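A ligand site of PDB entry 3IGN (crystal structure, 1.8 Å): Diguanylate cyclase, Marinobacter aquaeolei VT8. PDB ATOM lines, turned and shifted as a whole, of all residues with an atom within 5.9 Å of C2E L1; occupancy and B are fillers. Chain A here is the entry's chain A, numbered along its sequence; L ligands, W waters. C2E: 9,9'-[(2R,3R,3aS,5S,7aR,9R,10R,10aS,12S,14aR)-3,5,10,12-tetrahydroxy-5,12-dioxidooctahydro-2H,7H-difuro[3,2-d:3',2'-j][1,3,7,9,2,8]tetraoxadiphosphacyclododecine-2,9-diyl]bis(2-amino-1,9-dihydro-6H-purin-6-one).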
ATOM      1  N   ASN A  76      20.314  30.289 -13.118  1.00  0.00           N
ATOM      2  CA  ASN A  76      18.930  29.846 -13.235  1.00  0.00           C
ATOM      3  C   ASN A  76      18.165  30.395 -14.436  1.00  0.00           C
ATOM      4  O   ASN A  76      17.011  30.035 -14.655  1.00  0.00           O
ATOM      5  CB  ASN A  76      18.159  30.202 -11.956  1.00  0.00           C
ATOM      6  CG  ASN A  76      18.186  29.087 -10.935  1.00  0.00           C
ATOM      7  OD1 ASN A  76      17.373  28.156 -11.004  1.00  0.00           O
ATOM      8  ND2 ASN A  76      19.112  29.168  -9.982  1.00  0.00           N
ATOM      9  N   ILE A  77      18.790  31.265 -15.223  1.00  0.00           N
ATOM     10  CA  ILE A  77      18.118  31.834 -16.381  1.00  0.00           C
ATOM     11  C   ILE A  77      18.770  31.406 -17.690  1.00  0.00           C
ATOM     12  O   ILE A  77      19.924  30.980 -17.709  1.00  0.00           O
ATOM     13  CB  ILE A  77      18.091  33.380 -16.324  1.00  0.00           C
ATOM     14  CG1 ILE A  77      19.503  33.944 -16.497  1.00  0.00           C
ATOM     15  CG2 ILE A  77      17.484  33.846 -15.012  1.00  0.00           C
ATOM     16  CD1 ILE A  77      19.573  35.457 -16.511  1.00  0.00           C
ATOM     17  N   ARG A  78      18.037  31.540 -18.783  1.00  0.00           N
ATOM     18  CA  ARG A  78      18.520  31.175 -20.108  1.00  0.00           C
ATOM     19  C   ARG A  78      19.527  32.206 -20.602  1.00  0.00           C
ATOM     20  O   ARG A  78      19.469  33.360 -20.212  1.00  0.00           O
ATOM     21  CB  ARG A  78      17.352  31.089 -21.096  1.00  0.00           C
ATOM     22  CG  ARG A  78      16.300  30.080 -20.677  1.00  0.00           C
ATOM     23  CD  ARG A  78      15.059  30.111 -21.558  1.00  0.00           C
ATOM     24  NE  ARG A  78      14.193  28.982 -21.195  1.00  0.00           N
ATOM     25  CZ  ARG A  78      13.033  28.701 -21.780  1.00  0.00           C
ATOM     26  NH1 ARG A  78      12.577  29.453 -22.765  1.00  0.00           N
ATOM     27  NH2 ARG A  78      12.339  27.652 -21.379  1.00  0.00           N
ATOM     28  N   SER A  80      19.540  33.449 -23.281  1.00  0.00           N
ATOM     29  CA  SER A  80      18.772  34.403 -24.072  1.00  0.00           C
ATOM     30  C   SER A  80      18.030  35.421 -23.202  1.00  0.00           C
ATOM     31  O   SER A  80      17.508  36.408 -23.707  1.00  0.00           O
ATOM     32  CB  SER A  80      17.806  33.654 -24.992  1.00  0.00           C
ATOM     33  OG  SER A  80      17.203  32.556 -24.318  1.00  0.00           O
ATOM     34  N   ASP A  81      17.964  35.162 -21.894  1.00  0.00           N
ATOM     35  CA  ASP A  81      17.345  36.100 -20.948  1.00  0.00           C
ATOM     36  C   ASP A  81      18.471  37.057 -20.578  1.00  0.00           C
ATOM     37  O   ASP A  81      19.639  36.676 -20.659  1.00  0.00           O
ATOM     38  CB  ASP A  81      16.869  35.385 -19.670  1.00  0.00           C
ATOM     39  CG  ASP A  81      15.723  34.412 -19.915  1.00  0.00           C
ATOM     40  OD1 ASP A  81      14.859  34.692 -20.769  1.00  0.00           O
ATOM     41  OD2 ASP A  81      15.676  33.380 -19.217  1.00  0.00           O
ATOM     42  N   LEU A  95      12.956  38.933 -20.190  1.00  0.00           N
ATOM     43  CA  LEU A  95      12.602  37.578 -20.591  1.00  0.00           C
ATOM     44  C   LEU A  95      11.920  37.623 -21.956  1.00  0.00           C
ATOM     45  O   LEU A  95      10.703  37.769 -22.043  1.00  0.00           O
ATOM     46  CB  LEU A  95      11.674  36.950 -19.555  1.00  0.00           C
ATOM     47  CG  LEU A  95      12.135  36.955 -18.090  1.00  0.00           C
ATOM     48  CD1 LEU A  95      11.021  36.407 -17.213  1.00  0.00           C
ATOM     49  CD2 LEU A  95      13.405  36.115 -17.927  1.00  0.00           C
ATOM     50  N   PRO A  96      12.692  37.494 -23.042  1.00  0.00           N
ATOM     51  CA  PRO A  96      12.090  37.527 -24.373  1.00  0.00           C
ATOM     52  C   PRO A  96      11.304  36.259 -24.677  1.00  0.00           C
ATOM     53  O   PRO A  96      11.582  35.193 -24.131  1.00  0.00           O
ATOM     54  CB  PRO A  96      13.312  37.697 -25.287  1.00  0.00           C
ATOM     55  CG  PRO A  96      14.358  36.912 -24.563  1.00  0.00           C
ATOM     56  CD  PRO A  96      14.158  37.339 -23.122  1.00  0.00           C
ATOM     57  N   GLU A  97      10.313  36.393 -25.563  1.00  0.00           N
ATOM     58  CA  GLU A  97       9.477  35.275 -25.992  1.00  0.00           C
ATOM     59  C   GLU A  97       8.863  34.561 -24.809  1.00  0.00           C
ATOM     60  O   GLU A  97       8.615  33.351 -24.866  1.00  0.00           O
ATOM     61  CB  GLU A  97      10.320  34.291 -26.792  1.00  0.00           C
ATOM     62  CG  GLU A  97      10.850  34.818 -28.107  1.00  0.00           C
ATOM     63  CD  GLU A  97       9.733  35.090 -29.103  1.00  0.00           C
ATOM     64  OE1 GLU A  97       8.740  34.329 -29.097  1.00  0.00           O
ATOM     65  OE2 GLU A  97       9.859  36.033 -29.894  1.00  0.00           O
ATOM     66  N   THR A  98       8.574  35.309 -23.754  1.00  0.00           N
ATOM     67  CA  THR A  98       8.042  34.738 -22.530  1.00  0.00           C
ATOM     68  C   THR A  98       6.868  35.555 -22.011  1.00  0.00           C
ATOM     69  O   THR A  98       7.025  36.749 -21.751  1.00  0.00           O
ATOM     70  CB  THR A  98       9.140  34.708 -21.448  1.00  0.00           C
ATOM     71  OG1 THR A  98      10.290  34.016 -21.965  1.00  0.00           O
ATOM     72  CG2 THR A  98       8.650  34.008 -20.178  1.00  0.00           C
ATOM     73  N   GLU A 101       2.645  34.332 -17.471  1.00  0.00           N
ATOM     74  CA  GLU A 101       2.545  33.057 -16.781  1.00  0.00           C
ATOM     75  C   GLU A 101       3.854  32.270 -16.829  1.00  0.00           C
ATOM     76  O   GLU A 101       4.207  31.609 -15.852  1.00  0.00           O
ATOM     77  CB  GLU A 101       1.406  32.230 -17.390  1.00  0.00           C
ATOM     78  CG  GLU A 101       0.002  32.850 -17.213  1.00  0.00           C
ATOM     79  CD  GLU A 101      -0.120  34.289 -17.729  1.00  0.00           C
ATOM     80  OE1 GLU A 101       0.349  34.585 -18.858  1.00  0.00           O
ATOM     81  OE2 GLU A 101      -0.715  35.120 -17.005  1.00  0.00           O
ATOM     82  N   SER A 102       4.572  32.343 -17.951  1.00  0.00           N
ATOM     83  CA  SER A 102       5.833  31.624 -18.094  1.00  0.00           C
ATOM     84  C   SER A 102       6.918  32.295 -17.254  1.00  0.00           C
ATOM     85  O   SER A 102       7.810  31.623 -16.735  1.00  0.00           O
ATOM     86  CB  SER A 102       6.257  31.579 -19.560  1.00  0.00           C
ATOM     87  OG  SER A 102       5.333  30.826 -20.307  1.00  0.00           O
ATOM     88  N   ALA A 103       6.849  33.616 -17.170  1.00  0.00           N
ATOM     89  CA  ALA A 103       7.816  34.370 -16.374  1.00  0.00           C
ATOM     90  C   ALA A 103       7.714  33.966 -14.903  1.00  0.00           C
ATOM     91  O   ALA A 103       8.714  33.855 -14.196  1.00  0.00           O
ATOM     92  CB  ALA A 103       7.560  35.867 -16.528  1.00  0.00           C
ATOM     93  N   VAL A 105       7.164  31.143 -13.703  1.00  0.00           N
ATOM     94  CA  VAL A 105       7.889  29.892 -13.507  1.00  0.00           C
ATOM     95  C   VAL A 105       9.371  30.107 -13.200  1.00  0.00           C
ATOM     96  O   VAL A 105       9.882  29.576 -12.225  1.00  0.00           O
ATOM     97  CB  VAL A 105       7.770  28.951 -14.734  1.00  0.00           C
ATOM     98  CG1 VAL A 105       8.610  27.709 -14.515  1.00  0.00           C
ATOM     99  CG2 VAL A 105       6.318  28.600 -14.978  1.00  0.00           C
ATOM    100  N   ILE A 106      10.052  30.883 -14.035  1.00  0.00           N
ATOM    101  CA  ILE A 106      11.461  31.140 -13.806  1.00  0.00           C
ATOM    102  C   ILE A 106      11.626  31.954 -12.524  1.00  0.00           C
ATOM    103  O   ILE A 106      12.540  31.719 -11.737  1.00  0.00           O
ATOM    104  CB  ILE A 106      12.106  31.896 -15.025  1.00  0.00           C
ATOM    105  CG1 ILE A 106      13.265  32.799 -14.568  1.00  0.00           C
ATOM    106  CG2 ILE A 106      11.065  32.707 -15.758  1.00  0.00           C
ATOM    107  CD1 ILE A 106      14.544  32.062 -14.220  1.00  0.00           C
ATOM    108  N   ARG A 109      11.260  29.672  -9.547  1.00  0.00           N
ATOM    109  CA  ARG A 109      12.428  28.818  -9.436  1.00  0.00           C
ATOM    110  C   ARG A 109      13.550  29.598  -8.751  1.00  0.00           C
ATOM    111  O   ARG A 109      14.252  29.058  -7.906  1.00  0.00           O
ATOM    112  CB  ARG A 109      12.876  28.329 -10.816  1.00  0.00           C
ATOM    113  CG  ARG A 109      13.866  27.171 -10.764  1.00  0.00           C
ATOM    114  CD  ARG A 109      14.072  26.537 -12.146  1.00  0.00           C
ATOM    115  NE  ARG A 109      14.712  27.455 -13.076  1.00  0.00           N
ATOM    116  CZ  ARG A 109      14.137  27.917 -14.185  1.00  0.00           C
ATOM    117  NH1 ARG A 109      12.908  27.550 -14.492  1.00  0.00           N
ATOM    118  NH2 ARG A 109      14.795  28.748 -14.977  1.00  0.00           N
HETATM  119  P1  C2E L   1       8.898  24.028 -16.855  1.00  0.00           P
HETATM  120  O2P C2E L   1      10.257  24.553 -16.173  1.00  0.00           O
HETATM  121  O1P C2E L   1       7.895  23.750 -15.802  1.00  0.00           O
HETATM  122  O5' C2E L   1       8.308  25.107 -17.858  1.00  0.00           O
HETATM  123  C5' C2E L   1       8.428  26.456 -17.630  1.00  0.00           C
HETATM  124  C4' C2E L   1       7.842  27.309 -18.749  1.00  0.00           C
HETATM  125  O4' C2E L   1       8.079  28.651 -18.314  1.00  0.00           O
HETATM  126  C3' C2E L   1       8.590  27.093 -20.097  1.00  0.00           C
HETATM  127  O3' C2E L   1       7.828  26.625 -21.223  1.00  0.00           O
HETATM  128  C2' C2E L   1       9.305  28.406 -20.345  1.00  0.00           C
HETATM  129  O2' C2E L   1       8.943  28.944 -21.614  1.00  0.00           O
HETATM  130  C1' C2E L   1       9.027  29.320 -19.166  1.00  0.00           C
HETATM  131  N9  C2E L   1      10.369  29.394 -18.536  1.00  0.00           N
HETATM  132  C8  C2E L   1      10.870  28.576 -17.544  1.00  0.00           C
HETATM  133  N7  C2E L   1      12.069  28.890 -17.233  1.00  0.00           N
HETATM  134  C5  C2E L   1      12.455  29.930 -17.997  1.00  0.00           C
HETATM  135  C6  C2E L   1      13.640  30.682 -18.111  1.00  0.00           C
HETATM  136  O6  C2E L   1      14.617  30.428 -17.416  1.00  0.00           O
HETATM  137  N1  C2E L   1      13.680  31.705 -19.028  1.00  0.00           N
HETATM  138  C2  C2E L   1      12.585  31.996 -19.814  1.00  0.00           C
HETATM  139  N2  C2E L   1      12.657  33.027 -20.714  1.00  0.00           N
HETATM  140  N3  C2E L   1      11.464  31.295 -19.718  1.00  0.00           N
HETATM  141  C4  C2E L   1      11.362  30.270 -18.840  1.00  0.00           C
HETATM  142  P11 C2E L   1       8.737  25.590 -22.075  1.00  0.00           P
HETATM  143  O21 C2E L   1      10.120  26.264 -22.576  1.00  0.00           O
HETATM  144  O11 C2E L   1       7.983  25.107 -23.246  1.00  0.00           O
HETATM  145  O5A C2E L   1       9.012  24.402 -21.048  1.00  0.00           O
HETATM  146  C5A C2E L   1       9.873  23.364 -21.304  1.00  0.00           C
HETATM  147  C4A C2E L   1       9.904  22.351 -20.152  1.00  0.00           C
HETATM  148  O4A C2E L   1      10.969  21.450 -20.477  1.00  0.00           O
HETATM  149  C3A C2E L   1      10.194  22.993 -18.773  1.00  0.00           C
HETATM  150  O3A C2E L   1       9.234  22.755 -17.783  1.00  0.00           O
HETATM  151  C2A C2E L   1      11.556  22.491 -18.374  1.00  0.00           C
HETATM  152  O2A C2E L   1      11.540  21.819 -17.102  1.00  0.00           O
HETATM  153  C1A C2E L   1      12.051  21.601 -19.499  1.00  0.00           C
HETATM  154  N91 C2E L   1      13.170  22.454 -19.990  1.00  0.00           N
HETATM  155  C81 C2E L   1      13.153  23.332 -21.060  1.00  0.00           C
HETATM  156  N71 C2E L   1      14.292  23.927 -21.172  1.00  0.00           N
HETATM  157  C51 C2E L   1      15.119  23.494 -20.207  1.00  0.00           C
HETATM  158  C61 C2E L   1      16.470  23.791 -19.838  1.00  0.00           C
HETATM  159  O61 C2E L   1      17.117  24.600 -20.474  1.00  0.00           O
HETATM  160  N11 C2E L   1      17.009  23.145 -18.758  1.00  0.00           N
HETATM  161  C21 C2E L   1      16.278  22.226 -18.046  1.00  0.00           C
HETATM  162  N21 C2E L   1      16.849  21.588 -16.971  1.00  0.00           N
HETATM  163  N31 C2E L   1      15.026  21.939 -18.373  1.00  0.00           N
HETATM  164  C41 C2E L   1      14.410  22.539 -19.429  1.00  0.00           C
HETATM  165  P1  C2E L   2      20.576  27.868 -21.444  1.00  0.00           P
HETATM  166  O2P C2E L   2      19.099  28.087 -22.060  1.00  0.00           O
HETATM  167  O1P C2E L   2      21.371  29.086 -21.548  1.00  0.00           O
HETATM  168  O5' C2E L   2      20.503  27.434 -19.911  1.00  0.00           O
HETATM  169  C5' C2E L   2      19.563  27.889 -19.028  1.00  0.00           C
HETATM  170  C4' C2E L   2      19.813  27.350 -17.618  1.00  0.00           C
HETATM  171  O4' C2E L   2      18.742  27.881 -16.829  1.00  0.00           O
HETATM  172  C3' C2E L   2      19.718  25.809 -17.586  1.00  0.00           C
HETATM  173  O3' C2E L   2      20.852  25.063 -17.136  1.00  0.00           O
HETATM  174  C2' C2E L   2      18.449  25.498 -16.808  1.00  0.00           C
HETATM  175  O2' C2E L   2      18.653  24.603 -15.707  1.00  0.00           O
HETATM  176  C1' C2E L   2      17.826  26.838 -16.418  1.00  0.00           C
HETATM  177  N9  C2E L   2      16.610  26.835 -17.247  1.00  0.00           N
HETATM  178  C8  C2E L   2      16.412  27.492 -18.429  1.00  0.00           C
HETATM  179  N7  C2E L   2      15.245  27.261 -18.909  1.00  0.00           N
HETATM  180  C5  C2E L   2      14.589  26.453 -18.067  1.00  0.00           C
HETATM  181  C6  C2E L   2      13.302  25.877 -18.072  1.00  0.00           C
HETATM  182  O6  C2E L   2      12.535  26.089 -18.989  1.00  0.00           O
HETATM  183  N1  C2E L   2      12.943  25.066 -17.027  1.00  0.00           N
HETATM  184  C2  C2E L   2      13.820  24.822 -15.984  1.00  0.00           C
HETATM  185  N2  C2E L   2      13.424  24.012 -14.956  1.00  0.00           N
HETATM  186  N3  C2E L   2      15.034  25.354 -15.969  1.00  0.00           N
HETATM  187  C4  C2E L   2      15.455  26.166 -16.975  1.00  0.00           C
HETATM  188  P11 C2E L   2      20.977  23.708 -17.993  1.00  0.00           P
HETATM  189  O21 C2E L   2      19.646  22.800 -17.909  1.00  0.00           O
HETATM  190  O11 C2E L   2      22.131  22.904 -17.527  1.00  0.00           O
HETATM  191  O5A C2E L   2      21.208  24.201 -19.466  1.00  0.00           O
HETATM  192  C5A C2E L   2      21.204  23.359 -20.533  1.00  0.00           C
HETATM  193  C4A C2E L   2      21.478  24.116 -21.819  1.00  0.00           C
HETATM  194  O4A C2E L   2      21.256  23.177 -22.864  1.00  0.00           O
HETATM  195  C3A C2E L   2      20.573  25.353 -22.019  1.00  0.00           C
HETATM  196  O3A C2E L   2      21.258  26.588 -22.178  1.00  0.00           O
HETATM  197  C2A C2E L   2      19.709  25.001 -23.194  1.00  0.00           C
HETATM  198  O2A C2E L   2      19.868  25.962 -24.240  1.00  0.00           O
HETATM  199  C1A C2E L   2      20.088  23.598 -23.637  1.00  0.00           C
HETATM  200  N91 C2E L   2      18.863  22.860 -23.249  1.00  0.00           N
HETATM  201  C81 C2E L   2      18.698  21.978 -22.196  1.00  0.00           C
HETATM  202  N71 C2E L   2      17.477  21.545 -22.142  1.00  0.00           N
HETATM  203  C51 C2E L   2      16.769  22.099 -23.134  1.00  0.00           C
HETATM  204  C61 C2E L   2      15.418  22.001 -23.563  1.00  0.00           C
HETATM  205  O61 C2E L   2      14.634  21.287 -22.966  1.00  0.00           O
HETATM  206  N11 C2E L   2      15.016  22.730 -24.658  1.00  0.00           N
HETATM  207  C21 C2E L   2      15.910  23.536 -25.327  1.00  0.00           C
HETATM  208  N21 C2E L   2      15.482  24.249 -26.417  1.00  0.00           N
HETATM  209  N31 C2E L   2      17.174  23.640 -24.927  1.00  0.00           N
HETATM  210  C41 C2E L   2      17.636  22.949 -23.869  1.00  0.00           C
HETATM  211  O   HOH W   1      10.048  28.714 -24.156  1.00  0.00           O
HETATM  212  O   HOH W   2      11.187  25.539 -13.582  1.00  0.00           O
HETATM  213  O   HOH W   3      14.857  33.757 -23.176  1.00  0.00           O
HETATM  214  O   HOH W   4       5.452  28.277 -21.852  1.00  0.00           O
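O21 of C2E L2 sits at hydrogen-bond distance from N11 of C2E L1 (2.8 Å).
Water W1 lies within hydrogen-bond range of an oxygen (O2') of C2E L1 (2.8 Å) and the guanidinium group (NH1) of Arg 78 (3.0 Å). Water W2 lies within hydrogen-bond range of NH1 of Arg 109 (2.8 Å), O2P of C2E L1 (2.9 Å) and N2 of C2E L2 (3.0 Å). Water W4 lies within hydrogen-bond range of O3' of C2E L1 and OG of Ser 102. Water W3 lies within hydrogen-bond range of OD1 of Asp 81 (2.6 Å), OG of Ser 80 (2.9 Å) and N2 of C2E L1 (3.4 Å).
OD2 of Asp 81 sits at hydrogen-bond distance from N of Arg 78 (3.0 Å). The guanidinium group (NH2) of Arg 109 sits at hydrogen-bond distance from the backbone carbonyl oxygen (O) of Asn 76, at 2.6 Å. The backbone carbonyl oxygen (O) of Pro 96 sits at hydrogen-bond distance from the side-chain hydroxyl (OG1) of Thr 98 (2.8 Å).
The side-chain carboxylate (OD2) of Asp 81 lies within hydrogen-bond range of a nitrogen (N1) of C2E L1. An oxygen (O6) of C2E L2 lies within hydrogen-bond range of the guanidinium group (NH2) of Arg 78, at 2.9 Å. N2 of C2E L1 lies within hydrogen-bond range of OG1 of Thr 98 (2.9 Å). An oxygen (O6) of C2E L1 sits at hydrogen-bond distance from the guanidinium group (NH2) of Arg 109. NH2 of Arg 78 lies within salt-bridge range of O21 of C2E L1, at 2.9 Å. The guanidinium group (NH1) of Arg 109 sits close to a nitrogen (N3) of C2E L2.
The backbone carbonyl oxygen (O) of Ser 102 sits close to an oxygen (O4') of C2E L1, 3.4 Å away. Merely in contact with C2E L1: Val 105, Ile 106, Asn 76 and Ile 77. Hydrophobic or aromatic side chains within 4 Å of C2E L1: Val 105 and Ile 106. Of the 15 residues printed, 9 come within 4 Å of C2E L1. The nearest printed residue that does not touch C2E L1 is Pro 96 (4.2 Å).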
